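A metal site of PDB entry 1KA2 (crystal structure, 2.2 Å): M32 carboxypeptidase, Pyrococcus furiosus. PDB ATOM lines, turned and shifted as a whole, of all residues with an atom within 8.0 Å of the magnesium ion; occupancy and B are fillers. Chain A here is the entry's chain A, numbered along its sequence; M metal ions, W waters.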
ATOM      1  N   PRO A 239      20.567  23.716  10.729  1.00  0.00           N
ATOM      2  CA  PRO A 239      22.024  23.588  10.822  1.00  0.00           C
ATOM      3  C   PRO A 239      22.695  24.900  11.202  1.00  0.00           C
ATOM      4  O   PRO A 239      22.354  25.950  10.670  1.00  0.00           O
ATOM      5  CB  PRO A 239      22.427  23.151   9.422  1.00  0.00           C
ATOM      6  CG  PRO A 239      21.230  22.412   8.932  1.00  0.00           C
ATOM      7  CD  PRO A 239      20.086  23.272   9.410  1.00  0.00           C
ATOM      8  N   PHE A 240      23.647  24.822  12.129  1.00  0.00           N
ATOM      9  CA  PHE A 240      24.408  25.989  12.538  1.00  0.00           C
ATOM     10  C   PHE A 240      25.755  25.568  13.086  1.00  0.00           C
ATOM     11  O   PHE A 240      26.030  24.374  13.232  1.00  0.00           O
ATOM     12  CB  PHE A 240      23.630  26.810  13.586  1.00  0.00           C
ATOM     13  CG  PHE A 240      23.451  26.104  14.916  1.00  0.00           C
ATOM     14  CD1 PHE A 240      24.431  26.179  15.890  1.00  0.00           C
ATOM     15  CD2 PHE A 240      22.301  25.373  15.170  1.00  0.00           C
ATOM     16  CE1 PHE A 240      24.258  25.515  17.114  1.00  0.00           C
ATOM     17  CE2 PHE A 240      22.129  24.715  16.381  1.00  0.00           C
ATOM     18  CZ  PHE A 240      23.115  24.786  17.362  1.00  0.00           C
ATOM     19  N   THR A 241      26.603  26.546  13.368  1.00  0.00           N
ATOM     20  CA  THR A 241      27.932  26.306  13.902  1.00  0.00           C
ATOM     21  C   THR A 241      28.109  27.201  15.114  1.00  0.00           C
ATOM     22  O   THR A 241      27.699  28.353  15.096  1.00  0.00           O
ATOM     23  CB  THR A 241      29.023  26.667  12.857  1.00  0.00           C
ATOM     24  OG1 THR A 241      28.980  25.755  11.765  1.00  0.00           O
ATOM     25  CG2 THR A 241      30.412  26.647  13.497  1.00  0.00           C
ATOM     26  N   SER A 266      24.767  20.705   3.601  1.00  0.00           N
ATOM     27  CA  SER A 266      24.531  21.498   4.803  1.00  0.00           C
ATOM     28  C   SER A 266      25.621  21.210   5.826  1.00  0.00           C
ATOM     29  O   SER A 266      26.117  22.122   6.492  1.00  0.00           O
ATOM     30  CB  SER A 266      23.170  21.141   5.378  1.00  0.00           C
ATOM     31  OG  SER A 266      23.053  21.656   6.680  1.00  0.00           O
ATOM     32  N   HIS A 269      28.730  22.752   4.499  1.00  0.00           N
ATOM     33  CA  HIS A 269      28.576  24.207   4.667  1.00  0.00           C
ATOM     34  C   HIS A 269      29.014  24.565   6.081  1.00  0.00           C
ATOM     35  O   HIS A 269      29.923  25.365   6.287  1.00  0.00           O
ATOM     36  CB  HIS A 269      27.117  24.623   4.456  1.00  0.00           C
ATOM     37  CG  HIS A 269      26.872  26.097   4.619  1.00  0.00           C
ATOM     38  ND1 HIS A 269      27.044  26.992   3.589  1.00  0.00           N
ATOM     39  CD2 HIS A 269      26.444  26.823   5.686  1.00  0.00           C
ATOM     40  CE1 HIS A 269      26.716  28.211   4.014  1.00  0.00           C
ATOM     41  NE2 HIS A 269      26.350  28.127   5.284  1.00  0.00           N
ATOM     42  N   GLU A 270      28.366  23.952   7.082  1.00  0.00           N
ATOM     43  CA  GLU A 270      28.727  24.238   8.463  1.00  0.00           C
ATOM     44  C   GLU A 270      30.176  23.883   8.758  1.00  0.00           C
ATOM     45  O   GLU A 270      30.828  24.563   9.534  1.00  0.00           O
ATOM     46  CB  GLU A 270      27.785  23.503   9.428  1.00  0.00           C
ATOM     47  CG  GLU A 270      26.300  23.927   9.346  1.00  0.00           C
ATOM     48  CD  GLU A 270      26.091  25.450   9.267  1.00  0.00           C
ATOM     49  OE1 GLU A 270      26.691  26.206  10.069  1.00  0.00           O
ATOM     50  OE2 GLU A 270      25.295  25.884   8.410  1.00  0.00           O
ATOM     51  N   GLY A 272      32.624  24.338   6.943  1.00  0.00           N
ATOM     52  CA  GLY A 272      33.400  25.489   6.490  1.00  0.00           C
ATOM     53  C   GLY A 272      33.465  26.579   7.538  1.00  0.00           C
ATOM     54  O   GLY A 272      34.488  27.247   7.694  1.00  0.00           O
ATOM     55  N   HIS A 273      32.347  26.785   8.238  1.00  0.00           N
ATOM     56  CA  HIS A 273      32.288  27.777   9.299  1.00  0.00           C
ATOM     57  C   HIS A 273      33.194  27.338  10.438  1.00  0.00           C
ATOM     58  O   HIS A 273      33.977  28.127  10.978  1.00  0.00           O
ATOM     59  CB  HIS A 273      30.866  27.897   9.854  1.00  0.00           C
ATOM     60  CG  HIS A 273      29.919  28.661   8.985  1.00  0.00           C
ATOM     61  ND1 HIS A 273      30.116  29.985   8.662  1.00  0.00           N
ATOM     62  CD2 HIS A 273      28.745  28.308   8.420  1.00  0.00           C
ATOM     63  CE1 HIS A 273      29.099  30.415   7.937  1.00  0.00           C
ATOM     64  NE2 HIS A 273      28.254  29.409   7.776  1.00  0.00           N
ATOM     65  N   LEU A 295      30.198  38.251   9.291  1.00  0.00           N
ATOM     66  CA  LEU A 295      29.272  37.353   8.616  1.00  0.00           C
ATOM     67  C   LEU A 295      29.701  37.068   7.199  1.00  0.00           C
ATOM     68  O   LEU A 295      29.550  35.944   6.714  1.00  0.00           O
ATOM     69  CB  LEU A 295      27.869  37.954   8.557  1.00  0.00           C
ATOM     70  CG  LEU A 295      27.071  38.144   9.844  1.00  0.00           C
ATOM     71  CD1 LEU A 295      25.665  38.710   9.522  1.00  0.00           C
ATOM     72  CD2 LEU A 295      27.001  36.787  10.540  1.00  0.00           C
ATOM     73  N   HIS A 298      32.792  34.834   7.052  1.00  0.00           N
ATOM     74  CA  HIS A 298      32.387  33.503   7.506  1.00  0.00           C
ATOM     75  C   HIS A 298      31.669  32.755   6.398  1.00  0.00           C
ATOM     76  O   HIS A 298      31.930  31.589   6.161  1.00  0.00           O
ATOM     77  CB  HIS A 298      31.504  33.580   8.754  1.00  0.00           C
ATOM     78  CG  HIS A 298      32.083  32.866   9.945  1.00  0.00           C
ATOM     79  ND1 HIS A 298      32.175  31.494  10.012  1.00  0.00           N
ATOM     80  CD2 HIS A 298      32.610  33.343  11.094  1.00  0.00           C
ATOM     81  CE1 HIS A 298      32.740  31.157  11.161  1.00  0.00           C
ATOM     82  NE2 HIS A 298      33.018  32.254  11.832  1.00  0.00           N
ATOM     83  N   GLU A 299      30.774  33.438   5.690  1.00  0.00           N
ATOM     84  CA  GLU A 299      30.070  32.803   4.600  1.00  0.00           C
ATOM     85  C   GLU A 299      30.970  32.532   3.391  1.00  0.00           C
ATOM     86  O   GLU A 299      30.611  31.770   2.494  1.00  0.00           O
ATOM     87  CB  GLU A 299      28.846  33.639   4.197  1.00  0.00           C
ATOM     88  CG  GLU A 299      27.667  33.439   5.157  1.00  0.00           C
ATOM     89  CD  GLU A 299      26.974  32.105   4.963  1.00  0.00           C
ATOM     90  OE1 GLU A 299      26.167  31.949   4.040  1.00  0.00           O
ATOM     91  OE2 GLU A 299      27.227  31.156   5.704  1.00  0.00           O
ATOM     92  N   SER A 300      32.146  33.149   3.351  1.00  0.00           N
ATOM     93  CA  SER A 300      33.052  32.862   2.238  1.00  0.00           C
ATOM     94  C   SER A 300      33.668  31.476   2.504  1.00  0.00           C
ATOM     95  O   SER A 300      34.041  30.757   1.579  1.00  0.00           O
ATOM     96  CB  SER A 300      34.166  33.910   2.132  1.00  0.00           C
ATOM     97  OG  SER A 300      35.100  33.805   3.187  1.00  0.00           O
ATOM     98  N   GLN A 301      33.746  31.095   3.777  1.00  0.00           N
ATOM     99  CA  GLN A 301      34.324  29.808   4.152  1.00  0.00           C
ATOM    100  C   GLN A 301      33.302  28.692   4.002  1.00  0.00           C
ATOM    101  O   GLN A 301      33.602  27.648   3.425  1.00  0.00           O
ATOM    102  CB  GLN A 301      34.840  29.870   5.584  1.00  0.00           C
ATOM    103  CG  GLN A 301      35.937  30.887   5.745  1.00  0.00           C
ATOM    104  CD  GLN A 301      37.076  30.650   4.762  1.00  0.00           C
ATOM    105  OE1 GLN A 301      37.803  29.667   4.872  1.00  0.00           O
ATOM    106  NE2 GLN A 301      37.213  31.547   3.786  1.00  0.00           N
ATOM    107  N   SER A 302      32.093  28.923   4.510  1.00  0.00           N
ATOM    108  CA  SER A 302      31.048  27.917   4.398  1.00  0.00           C
ATOM    109  C   SER A 302      30.716  27.638   2.927  1.00  0.00           C
ATOM    110  O   SER A 302      30.540  26.488   2.546  1.00  0.00           O
ATOM    111  CB  SER A 302      29.788  28.380   5.136  1.00  0.00           C
ATOM    112  OG  SER A 302      29.248  29.564   4.570  1.00  0.00           O
ATOM    113  N   ARG A 303      30.624  28.692   2.123  1.00  0.00           N
ATOM    114  CA  ARG A 303      30.305  28.523   0.700  1.00  0.00           C
ATOM    115  C   ARG A 303      31.495  27.947  -0.060  1.00  0.00           C
ATOM    116  O   ARG A 303      31.323  27.279  -1.072  1.00  0.00           O
ATOM    117  CB  ARG A 303      29.889  29.852   0.073  1.00  0.00           C
ATOM    118  CG  ARG A 303      28.599  30.441   0.643  1.00  0.00           C
ATOM    119  CD  ARG A 303      27.402  29.514   0.407  1.00  0.00           C
ATOM    120  NE  ARG A 303      26.144  30.236   0.618  1.00  0.00           N
ATOM    121  CZ  ARG A 303      24.936  29.688   0.579  1.00  0.00           C
ATOM    122  NH1 ARG A 303      24.794  28.394   0.335  1.00  0.00           N
ATOM    123  NH2 ARG A 303      23.865  30.452   0.753  1.00  0.00           N
ATOM    124  N   GLU A 306      31.094  24.267   0.734  1.00  0.00           N
ATOM    125  CA  GLU A 306      29.836  23.756   0.196  1.00  0.00           C
ATOM    126  C   GLU A 306      29.740  23.725  -1.332  1.00  0.00           C
ATOM    127  O   GLU A 306      29.485  22.671  -1.916  1.00  0.00           O
ATOM    128  CB  GLU A 306      28.658  24.581   0.733  1.00  0.00           C
ATOM    129  CG  GLU A 306      27.312  24.101   0.211  1.00  0.00           C
ATOM    130  CD  GLU A 306      26.229  25.126   0.388  1.00  0.00           C
ATOM    131  OE1 GLU A 306      26.559  26.247   0.861  1.00  0.00           O
ATOM    132  OE2 GLU A 306      25.063  24.843   0.041  1.00  0.00           O
ATOM    133  N   TYR A 419      21.098  42.879   6.944  1.00  0.00           N
ATOM    134  CA  TYR A 419      21.783  41.605   7.168  1.00  0.00           C
ATOM    135  C   TYR A 419      21.921  40.752   5.897  1.00  0.00           C
ATOM    136  O   TYR A 419      22.995  40.218   5.608  1.00  0.00           O
ATOM    137  CB  TYR A 419      21.022  40.824   8.250  1.00  0.00           C
ATOM    138  CG  TYR A 419      21.637  39.502   8.658  1.00  0.00           C
ATOM    139  CD1 TYR A 419      22.166  39.321   9.937  1.00  0.00           C
ATOM    140  CD2 TYR A 419      21.625  38.426   7.787  1.00  0.00           C
ATOM    141  CE1 TYR A 419      22.652  38.086  10.332  1.00  0.00           C
ATOM    142  CE2 TYR A 419      22.114  37.204   8.157  1.00  0.00           C
ATOM    143  CZ  TYR A 419      22.622  37.029   9.430  1.00  0.00           C
ATOM    144  OH  TYR A 419      23.073  35.799   9.785  1.00  0.00           O
ATOM    145  N   TYR A 423      25.158  37.493   2.858  1.00  0.00           N
ATOM    146  CA  TYR A 423      25.096  36.149   2.238  1.00  0.00           C
ATOM    147  C   TYR A 423      25.709  36.178   0.833  1.00  0.00           C
ATOM    148  O   TYR A 423      26.465  35.270   0.453  1.00  0.00           O
ATOM    149  CB  TYR A 423      23.655  35.632   2.110  1.00  0.00           C
ATOM    150  CG  TYR A 423      22.980  35.209   3.417  1.00  0.00           C
ATOM    151  CD1 TYR A 423      22.110  36.059   4.085  1.00  0.00           C
ATOM    152  CD2 TYR A 423      23.187  33.925   3.940  1.00  0.00           C
ATOM    153  CE1 TYR A 423      21.444  35.657   5.236  1.00  0.00           C
ATOM    154  CE2 TYR A 423      22.525  33.510   5.094  1.00  0.00           C
ATOM    155  CZ  TYR A 423      21.652  34.386   5.735  1.00  0.00           C
ATOM    156  OH  TYR A 423      21.001  33.988   6.873  1.00  0.00           O
HETATM  157 MG    MG M   1      26.356  29.693   7.000  1.00  0.00          MG
HETATM  158  O   HOH W   1      24.472  30.240   5.928  1.00  0.00           O
HETATM  159  O   HOH W   2      25.652  31.294   8.276  1.00  0.00           O
HETATM  160  O   HOH W   3      25.206  28.468   8.418  1.00  0.00           O
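The magnesium ion is bound by NE2 of His 273, 2.1 Å away. The side-chain carboxylate (OE2) of Glu 299 is bound to the magnesium ion (2.1 Å). The magnesium ion is bound by water W2 (2.2 Å). Water W3 is bound to the magnesium ion (2.2 Å). The magnesium ion is bound by water W1. NE2 of His 269 binds the magnesium ion.
A ring nitrogen (NE2) of His 273 sits close to the side-chain hydroxyl (OG) of Ser 302, 3.4 Å away. ND1 of His 273 lies within hydrogen-bond range of ND1 of His 298, 2.9 Å away. OG of Ser 302 is in hydrogen-bond range of O of Glu 299. The side-chain carboxylate of Glu 299 is in salt-bridge range of the guanidinium group of Arg 303 (3.8 Å). A ring nitrogen (NE2) of His 269 lies close to the side-chain hydroxyl (OG) of Ser 302 (3.3 Å). ND1 of His 269 is in hydrogen-bond range of OE1 of Glu 306, at 2.9 Å.
Ser 302 touches the magnesium ion. Within 4 Å of the magnesium ion: His 269, His 273, Glu 299 and Ser 302. The nearest printed residue that does not touch the magnesium ion is Glu 270 (4.2 Å).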
